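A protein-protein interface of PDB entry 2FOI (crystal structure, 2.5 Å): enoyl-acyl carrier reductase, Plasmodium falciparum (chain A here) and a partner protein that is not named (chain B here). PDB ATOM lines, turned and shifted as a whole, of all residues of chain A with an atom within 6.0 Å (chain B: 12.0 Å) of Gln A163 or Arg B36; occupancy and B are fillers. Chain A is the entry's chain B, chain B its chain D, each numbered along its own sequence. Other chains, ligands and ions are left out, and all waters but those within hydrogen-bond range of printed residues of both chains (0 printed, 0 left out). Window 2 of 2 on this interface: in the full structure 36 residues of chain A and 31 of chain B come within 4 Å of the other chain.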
ATOM      1  N   ASN A 114       5.129   8.767 -13.106  1.00  0.00           N
ATOM      2  CA  ASN A 114       3.716   8.979 -13.399  1.00  0.00           C
ATOM      3  C   ASN A 114       3.379   9.052 -14.871  1.00  0.00           C
ATOM      4  O   ASN A 114       2.234   9.290 -15.231  1.00  0.00           O
ATOM      5  CB  ASN A 114       3.204  10.225 -12.692  1.00  0.00           C
ATOM      6  CG  ASN A 114       4.077  11.404 -12.945  1.00  0.00           C
ATOM      7  OD1 ASN A 114       4.697  11.506 -14.004  1.00  0.00           O
ATOM      8  ND2 ASN A 114       4.171  12.293 -11.966  1.00  0.00           N
ATOM      9  N   MET A 115       4.378   8.861 -15.717  1.00  0.00           N
ATOM     10  CA  MET A 115       4.152   8.812 -17.140  1.00  0.00           C
ATOM     11  C   MET A 115       4.942   7.655 -17.721  1.00  0.00           C
ATOM     12  O   MET A 115       6.090   7.415 -17.334  1.00  0.00           O
ATOM     13  CB  MET A 115       4.563  10.122 -17.771  1.00  0.00           C
ATOM     14  CG  MET A 115       3.650  11.261 -17.372  1.00  0.00           C
ATOM     15  SD  MET A 115       4.340  12.807 -17.947  1.00  0.00           S
ATOM     16  CE  MET A 115       3.184  13.972 -17.205  1.00  0.00           C
ATOM     17  N   LYS A 161       2.261   6.551  -9.556  1.00  0.00           N
ATOM     18  CA  LYS A 161       1.313   7.127  -8.631  1.00  0.00           C
ATOM     19  C   LYS A 161      -0.105   6.972  -9.189  1.00  0.00           C
ATOM     20  O   LYS A 161      -0.284   6.778 -10.393  1.00  0.00           O
ATOM     21  CB  LYS A 161       1.656   8.599  -8.392  1.00  0.00           C
ATOM     22  CG  LYS A 161       3.137   8.827  -8.029  1.00  0.00           C
ATOM     23  CD  LYS A 161       3.377  10.201  -7.406  1.00  0.00           C
ATOM     24  CE  LYS A 161       4.839  10.626  -7.527  1.00  0.00           C
ATOM     25  NZ  LYS A 161       4.991  12.112  -7.466  1.00  0.00           N
ATOM     26  N   PRO A 162      -1.123   7.019  -8.315  1.00  0.00           N
ATOM     27  CA  PRO A 162      -2.456   7.094  -8.905  1.00  0.00           C
ATOM     28  C   PRO A 162      -2.508   8.358  -9.741  1.00  0.00           C
ATOM     29  O   PRO A 162      -1.741   9.290  -9.486  1.00  0.00           O
ATOM     30  CB  PRO A 162      -3.399   7.199  -7.687  1.00  0.00           C
ATOM     31  CG  PRO A 162      -2.509   7.589  -6.521  1.00  0.00           C
ATOM     32  CD  PRO A 162      -1.149   7.000  -6.839  1.00  0.00           C
ATOM     33  N   GLN A 163      -3.387   8.374 -10.742  1.00  0.00           N
ATOM     34  CA  GLN A 163      -3.527   9.515 -11.661  1.00  0.00           C
ATOM     35  C   GLN A 163      -2.487   9.551 -12.790  1.00  0.00           C
ATOM     36  O   GLN A 163      -2.532  10.410 -13.665  1.00  0.00           O
ATOM     37  CB  GLN A 163      -3.609  10.847 -10.899  1.00  0.00           C
ATOM     38  CG  GLN A 163      -4.971  11.015 -10.209  1.00  0.00           C
ATOM     39  CD  GLN A 163      -5.132  12.312  -9.405  1.00  0.00           C
ATOM     40  OE1 GLN A 163      -4.276  13.209  -9.423  1.00  0.00           O
ATOM     41  NE2 GLN A 163      -6.255  12.412  -8.700  1.00  0.00           N
ATOM     42  N   SER A 164      -1.572   8.594 -12.788  1.00  0.00           N
ATOM     43  CA  SER A 164      -0.604   8.516 -13.852  1.00  0.00           C
ATOM     44  C   SER A 164      -1.264   8.098 -15.161  1.00  0.00           C
ATOM     45  O   SER A 164      -2.428   7.626 -15.190  1.00  0.00           O
ATOM     46  CB  SER A 164       0.497   7.538 -13.487  1.00  0.00           C
ATOM     47  OG  SER A 164       1.048   7.863 -12.230  1.00  0.00           O
ATOM     48  N   SER A 165      -0.504   8.260 -16.246  1.00  0.00           N
ATOM     49  CA  SER A 165      -1.024   8.064 -17.592  1.00  0.00           C
ATOM     50  C   SER A 165      -0.024   7.326 -18.477  1.00  0.00           C
ATOM     51  O   SER A 165       1.180   7.561 -18.416  1.00  0.00           O
ATOM     52  CB  SER A 165      -1.395   9.419 -18.194  1.00  0.00           C
ATOM     53  OG  SER A 165      -1.903   9.258 -19.508  1.00  0.00           O
ATOM     54  N   TYR A 207      -6.385   1.283 -10.176  1.00  0.00           N
ATOM     55  CA  TYR A 207      -5.230   2.138  -9.889  1.00  0.00           C
ATOM     56  C   TYR A 207      -5.502   3.602 -10.132  1.00  0.00           C
ATOM     57  O   TYR A 207      -4.665   4.440  -9.830  1.00  0.00           O
ATOM     58  CB  TYR A 207      -4.009   1.714 -10.716  1.00  0.00           C
ATOM     59  CG  TYR A 207      -3.664   0.271 -10.541  1.00  0.00           C
ATOM     60  CD1 TYR A 207      -2.714  -0.134  -9.601  1.00  0.00           C
ATOM     61  CD2 TYR A 207      -4.302  -0.700 -11.280  1.00  0.00           C
ATOM     62  CE1 TYR A 207      -2.403  -1.476  -9.420  1.00  0.00           C
ATOM     63  CE2 TYR A 207      -4.006  -2.049 -11.099  1.00  0.00           C
ATOM     64  CZ  TYR A 207      -3.057  -2.427 -10.168  1.00  0.00           C
ATOM     65  OH  TYR A 207      -2.769  -3.765 -10.011  1.00  0.00           O
ATOM     66  N   ASN A 208      -6.656   3.919 -10.700  1.00  0.00           N
ATOM     67  CA  ASN A 208      -6.904   5.288 -11.141  1.00  0.00           C
ATOM     68  C   ASN A 208      -5.847   5.756 -12.164  1.00  0.00           C
ATOM     69  O   ASN A 208      -5.422   6.907 -12.149  1.00  0.00           O
ATOM     70  CB  ASN A 208      -6.967   6.251  -9.944  1.00  0.00           C
ATOM     71  CG  ASN A 208      -7.623   7.580 -10.307  1.00  0.00           C
ATOM     72  OD1 ASN A 208      -8.429   7.644 -11.233  1.00  0.00           O
ATOM     73  ND2 ASN A 208      -7.278   8.640  -9.587  1.00  0.00           N
ATOM     74  N   ILE A 209      -5.413   4.832 -13.028  1.00  0.00           N
ATOM     75  CA  ILE A 209      -4.417   5.098 -14.080  1.00  0.00           C
ATOM     76  C   ILE A 209      -5.069   4.961 -15.431  1.00  0.00           C
ATOM     77  O   ILE A 209      -5.913   4.094 -15.645  1.00  0.00           O
ATOM     78  CB  ILE A 209      -3.207   4.151 -13.965  1.00  0.00           C
ATOM     79  CG1 ILE A 209      -2.286   4.630 -12.827  1.00  0.00           C
ATOM     80  CG2 ILE A 209      -2.418   4.077 -15.263  1.00  0.00           C
ATOM     81  CD1 ILE A 209      -1.131   3.737 -12.603  1.00  0.00           C
ATOM     82  N   ARG A 210      -4.699   5.856 -16.329  1.00  0.00           N
ATOM     83  CA  ARG A 210      -5.303   5.949 -17.644  1.00  0.00           C
ATOM     84  C   ARG A 210      -4.352   5.441 -18.705  1.00  0.00           C
ATOM     85  O   ARG A 210      -3.115   5.576 -18.567  1.00  0.00           O
ATOM     86  CB  ARG A 210      -5.615   7.411 -17.957  1.00  0.00           C
ATOM     87  CG  ARG A 210      -6.499   8.092 -16.944  1.00  0.00           C
ATOM     88  CD  ARG A 210      -6.757   9.530 -17.323  1.00  0.00           C
ATOM     89  NE  ARG A 210      -5.542  10.347 -17.402  1.00  0.00           N
ATOM     90  CZ  ARG A 210      -5.046  10.850 -18.533  1.00  0.00           C
ATOM     91  NH1 ARG A 210      -5.662  10.594 -19.682  1.00  0.00           N
ATOM     92  NH2 ARG A 210      -3.946  11.623 -18.527  1.00  0.00           N
ATOM     93  N   SER B  28       3.519  16.171 -29.009  1.00  0.00           N
ATOM     94  CA  SER B  28       2.759  17.111 -28.221  1.00  0.00           C
ATOM     95  C   SER B  28       1.408  16.519 -27.854  1.00  0.00           C
ATOM     96  O   SER B  28       0.838  16.875 -26.842  1.00  0.00           O
ATOM     97  CB  SER B  28       2.565  18.418 -28.989  1.00  0.00           C
ATOM     98  OG  SER B  28       1.622  18.230 -30.036  1.00  0.00           O
ATOM     99  N   VAL B  29       0.878  15.633 -28.692  1.00  0.00           N
ATOM    100  CA  VAL B  29      -0.382  14.974 -28.362  1.00  0.00           C
ATOM    101  C   VAL B  29      -0.074  13.975 -27.260  1.00  0.00           C
ATOM    102  O   VAL B  29      -0.821  13.848 -26.288  1.00  0.00           O
ATOM    103  CB  VAL B  29      -0.958  14.256 -29.575  1.00  0.00           C
ATOM    104  CG1 VAL B  29      -2.279  13.590 -29.222  1.00  0.00           C
ATOM    105  CG2 VAL B  29      -1.140  15.221 -30.716  1.00  0.00           C
ATOM    106  N   ALA B  30       1.062  13.291 -27.390  1.00  0.00           N
ATOM    107  CA  ALA B  30       1.479  12.351 -26.358  1.00  0.00           C
ATOM    108  C   ALA B  30       1.552  13.088 -25.039  1.00  0.00           C
ATOM    109  O   ALA B  30       1.090  12.612 -24.011  1.00  0.00           O
ATOM    110  CB  ALA B  30       2.831  11.771 -26.697  1.00  0.00           C
ATOM    111  N   SER B  31       2.151  14.265 -25.091  1.00  0.00           N
ATOM    112  CA  SER B  31       2.354  15.106 -23.923  1.00  0.00           C
ATOM    113  C   SER B  31       1.017  15.465 -23.227  1.00  0.00           C
ATOM    114  O   SER B  31       0.877  15.371 -22.009  1.00  0.00           O
ATOM    115  CB  SER B  31       3.050  16.376 -24.389  1.00  0.00           C
ATOM    116  OG  SER B  31       3.328  17.234 -23.305  1.00  0.00           O
ATOM    117  N   PHE B  32       0.043  15.887 -24.014  1.00  0.00           N
ATOM    118  CA  PHE B  32      -1.285  16.190 -23.501  1.00  0.00           C
ATOM    119  C   PHE B  32      -1.983  14.957 -22.877  1.00  0.00           C
ATOM    120  O   PHE B  32      -2.567  15.029 -21.793  1.00  0.00           O
ATOM    121  CB  PHE B  32      -2.118  16.755 -24.641  1.00  0.00           C
ATOM    122  CG  PHE B  32      -3.580  16.644 -24.426  1.00  0.00           C
ATOM    123  CD1 PHE B  32      -4.227  17.474 -23.517  1.00  0.00           C
ATOM    124  CD2 PHE B  32      -4.327  15.721 -25.146  1.00  0.00           C
ATOM    125  CE1 PHE B  32      -5.601  17.385 -23.324  1.00  0.00           C
ATOM    126  CE2 PHE B  32      -5.699  15.627 -24.945  1.00  0.00           C
ATOM    127  CZ  PHE B  32      -6.332  16.467 -24.041  1.00  0.00           C
ATOM    128  N   LEU B  33      -1.921  13.828 -23.568  1.00  0.00           N
ATOM    129  CA  LEU B  33      -2.497  12.594 -23.030  1.00  0.00           C
ATOM    130  C   LEU B  33      -1.861  12.181 -21.711  1.00  0.00           C
ATOM    131  O   LEU B  33      -2.534  11.686 -20.806  1.00  0.00           O
ATOM    132  CB  LEU B  33      -2.344  11.471 -24.041  1.00  0.00           C
ATOM    133  CG  LEU B  33      -3.291  11.636 -25.216  1.00  0.00           C
ATOM    134  CD1 LEU B  33      -3.001  10.593 -26.309  1.00  0.00           C
ATOM    135  CD2 LEU B  33      -4.730  11.507 -24.699  1.00  0.00           C
ATOM    136  N   LEU B  34      -0.558  12.387 -21.610  1.00  0.00           N
ATOM    137  CA  LEU B  34       0.163  12.001 -20.406  1.00  0.00           C
ATOM    138  C   LEU B  34      -0.109  12.944 -19.257  1.00  0.00           C
ATOM    139  O   LEU B  34       0.021  12.573 -18.089  1.00  0.00           O
ATOM    140  CB  LEU B  34       1.660  11.960 -20.670  1.00  0.00           C
ATOM    141  CG  LEU B  34       2.005  10.750 -21.510  1.00  0.00           C
ATOM    142  CD1 LEU B  34       3.445  10.857 -22.019  1.00  0.00           C
ATOM    143  CD2 LEU B  34       1.747   9.494 -20.697  1.00  0.00           C
ATOM    144  N   SER B  35      -0.477  14.168 -19.586  1.00  0.00           N
ATOM    145  CA  SER B  35      -0.736  15.154 -18.559  1.00  0.00           C
ATOM    146  C   SER B  35      -2.155  15.033 -17.986  1.00  0.00           C
ATOM    147  O   SER B  35      -3.037  14.365 -18.537  1.00  0.00           O
ATOM    148  CB  SER B  35      -0.569  16.547 -19.153  1.00  0.00           C
ATOM    149  OG  SER B  35      -1.814  16.952 -19.697  1.00  0.00           O
ATOM    150  N   ARG B  36      -2.367  15.728 -16.889  1.00  0.00           N
ATOM    151  CA  ARG B  36      -3.671  15.845 -16.248  1.00  0.00           C
ATOM    152  C   ARG B  36      -4.736  16.504 -17.101  1.00  0.00           C
ATOM    153  O   ARG B  36      -5.916  16.332 -16.821  1.00  0.00           O
ATOM    154  CB  ARG B  36      -3.517  16.636 -14.941  1.00  0.00           C
ATOM    155  CG  ARG B  36      -2.727  15.846 -13.911  1.00  0.00           C
ATOM    156  CD  ARG B  36      -3.620  14.771 -13.288  1.00  0.00           C
ATOM    157  NE  ARG B  36      -4.615  15.414 -12.430  1.00  0.00           N
ATOM    158  CZ  ARG B  36      -5.787  14.893 -12.081  1.00  0.00           C
ATOM    159  NH1 ARG B  36      -6.149  13.687 -12.523  1.00  0.00           N
ATOM    160  NH2 ARG B  36      -6.594  15.603 -11.290  1.00  0.00           N
ATOM    161  N   GLU B  37      -4.340  17.271 -18.114  1.00  0.00           N
ATOM    162  CA  GLU B  37      -5.309  17.950 -18.972  1.00  0.00           C
ATOM    163  C   GLU B  37      -6.299  16.986 -19.643  1.00  0.00           C
ATOM    164  O   GLU B  37      -7.386  17.388 -20.110  1.00  0.00           O
ATOM    165  CB  GLU B  37      -4.578  18.735 -20.066  1.00  0.00           C
ATOM    166  CG  GLU B  37      -3.722  19.872 -19.555  1.00  0.00           C
ATOM    167  CD  GLU B  37      -4.517  20.817 -18.684  1.00  0.00           C
ATOM    168  OE1 GLU B  37      -4.496  20.646 -17.448  1.00  0.00           O
ATOM    169  OE2 GLU B  37      -5.185  21.714 -19.231  1.00  0.00           O
ATOM    170  N   SER B  38      -5.910  15.717 -19.716  1.00  0.00           N
ATOM    171  CA  SER B  38      -6.723  14.719 -20.365  1.00  0.00           C
ATOM    172  C   SER B  38      -7.274  13.725 -19.345  1.00  0.00           C
ATOM    173  O   SER B  38      -7.504  12.558 -19.671  1.00  0.00           O
ATOM    174  CB  SER B  38      -5.905  14.000 -21.441  1.00  0.00           C
ATOM    175  OG  SER B  38      -4.948  13.140 -20.866  1.00  0.00           O
ATOM    176  N   ARG B  39      -7.494  14.195 -18.117  1.00  0.00           N
ATOM    177  CA  ARG B  39      -7.888  13.299 -17.027  1.00  0.00           C
ATOM    178  C   ARG B  39      -9.178  12.502 -17.259  1.00  0.00           C
ATOM    179  O   ARG B  39      -9.371  11.481 -16.602  1.00  0.00           O
ATOM    180  CB  ARG B  39      -7.963  14.042 -15.691  1.00  0.00           C
ATOM    181  CG  ARG B  39      -9.100  15.043 -15.565  1.00  0.00           C
ATOM    182  CD  ARG B  39      -9.075  15.744 -14.201  1.00  0.00           C
ATOM    183  NE  ARG B  39      -9.261  14.819 -13.074  1.00  0.00           N
ATOM    184  CZ  ARG B  39     -10.373  14.711 -12.343  1.00  0.00           C
ATOM    185  NH1 ARG B  39     -11.447  15.467 -12.602  1.00  0.00           N
ATOM    186  NH2 ARG B  39     -10.403  13.841 -11.341  1.00  0.00           N
ATOM    187  N   ALA B  40     -10.044  12.954 -18.177  1.00  0.00           N
ATOM    188  CA  ALA B  40     -11.291  12.236 -18.490  1.00  0.00           C
ATOM    189  C   ALA B  40     -11.279  11.337 -19.748  1.00  0.00           C
ATOM    190  O   ALA B  40     -12.330  10.796 -20.133  1.00  0.00           O
ATOM    191  CB  ALA B  40     -12.472  13.185 -18.527  1.00  0.00           C
ATOM    192  N   ILE B  41     -10.106  11.188 -20.372  1.00  0.00           N
ATOM    193  CA  ILE B  41      -9.928  10.367 -21.571  1.00  0.00           C
ATOM    194  C   ILE B  41      -9.130   9.121 -21.235  1.00  0.00           C
ATOM    195  O   ILE B  41      -8.003   9.226 -20.735  1.00  0.00           O
ATOM    196  CB  ILE B  41      -9.109  11.095 -22.643  1.00  0.00           C
ATOM    197  CG1 ILE B  41      -9.683  12.481 -22.949  1.00  0.00           C
ATOM    198  CG2 ILE B  41      -9.058  10.264 -23.934  1.00  0.00           C
ATOM    199  CD1 ILE B  41      -8.978  13.138 -24.118  1.00  0.00           C
ATOM    200  N   THR B  42      -9.694   7.943 -21.516  1.00  0.00           N
ATOM    201  CA  THR B  42      -8.960   6.691 -21.315  1.00  0.00           C
ATOM    202  C   THR B  42      -9.536   5.627 -22.232  1.00  0.00           C
ATOM    203  O   THR B  42     -10.737   5.635 -22.530  1.00  0.00           O
ATOM    204  CB  THR B  42      -9.063   6.220 -19.851  1.00  0.00           C
ATOM    205  OG1 THR B  42      -8.050   5.245 -19.566  1.00  0.00           O
ATOM    206  CG2 THR B  42     -10.453   5.615 -19.567  1.00  0.00           C
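OG of Ser A165 is in hydrogen-bond range of O of Leu B33. The guanidinium group of Arg A210 sits at hydrogen-bond distance from the backbone carbonyl oxygen of Ser B35 (2.9 Å). The backbone carbonyl oxygen (O) of Ser B38 lies within hydrogen-bond range of the guanidinium group (NH1) of Arg A210 (2.7 Å). The guanidinium group of Arg A210 sits at hydrogen-bond distance from the backbone carbonyl oxygen of Leu B33 (2.7 Å). NH1 of Arg A210 sits at hydrogen-bond distance from O of Ile B41, at 2.9 Å.
OG of Ser B35 is in hydrogen-bond range of N of Glu B37, 3.0 Å away. O of Asn A208 lies within hydrogen-bond range of N of Gln A163 (2.9 Å). O of Ser B35 is in hydrogen-bond range of OG of Ser B38 (3.3 Å). N of Arg A210 is in hydrogen-bond range of O of Ser A164, 3.1 Å away. The backbone carbonyl oxygen (O) of Phe B32 is in hydrogen-bond range of the side-chain hydroxyl (OG) of Ser B35, at 2.9 Å. OG of Ser A165 is in hydrogen-bond range of NH2 of Arg A210 (3.3 Å).
Of the 15 printed residues of chain B, 8 touch a printed residue of chain A. Hydrophobic or aromatic side chains of chain B that line the printed part of chain A: Leu B34. Along chain B the printed residues that touch a printed residue of chain A span positions 33 to 42. Printed residues of chain A that touch a printed residue of chain B: Met A115, Gln A163, Ser A165 and Arg A210. Among the printed residues, 10 pairs touch across the chains. Among the printed residues, no Asp or Glu carboxylate lies within 4 Å of a Lys or Arg side-chain nitrogen of the other chain.
Printed residues of chain B within 4 Å of Gln A163: Arg B36. Of chain A, only Gln A163 (3.5 Å) comes within 4 Å of Arg B36. No residue of chain B comes within 4 Å of Asn A114. Of the printed residues of chain B, Ser A165 touches Leu B33 (2.8 Å) and Leu B34 (3.0 Å). No residue of chain B comes within 4 Å of Asn A208. No residue of chain B comes within 4 Å of Ile A209. Arg A210 touches just these residues of chain B: Leu B33 (2.7 Å), Ser B35 (2.9 Å), Ser B38 (2.7 Å), Arg B39 (3.3 Å), Ile B41 (2.9 Å) and Thr B42 (3.4 Å). Of the printed residues of chain A, Leu B34 touches Met A115 (3.6 Å) and Ser A165 (3.0 Å). Of the printed residues of chain A, Ile B41 touches Arg A210 (2.9 Å). Ala B40 touches none of the printed residues of chain A. The nearest residue of chain B that does not touch Gln A163 is Arg B39 (5.1 Å). The nearest residue of chain A that does not touch Arg B36 is Arg A210 (4.7 Å). The nearest printed residue of chain A that does not touch Ser B35 is Met A115 (4.3 Å).
Among the printed residues, merely in contact across the chains: Met A115 with Leu B34, Gln A163 with Arg B36, Ser A165 with Leu B34, Arg A210 with Arg B39 and Arg A210 with Thr B42.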
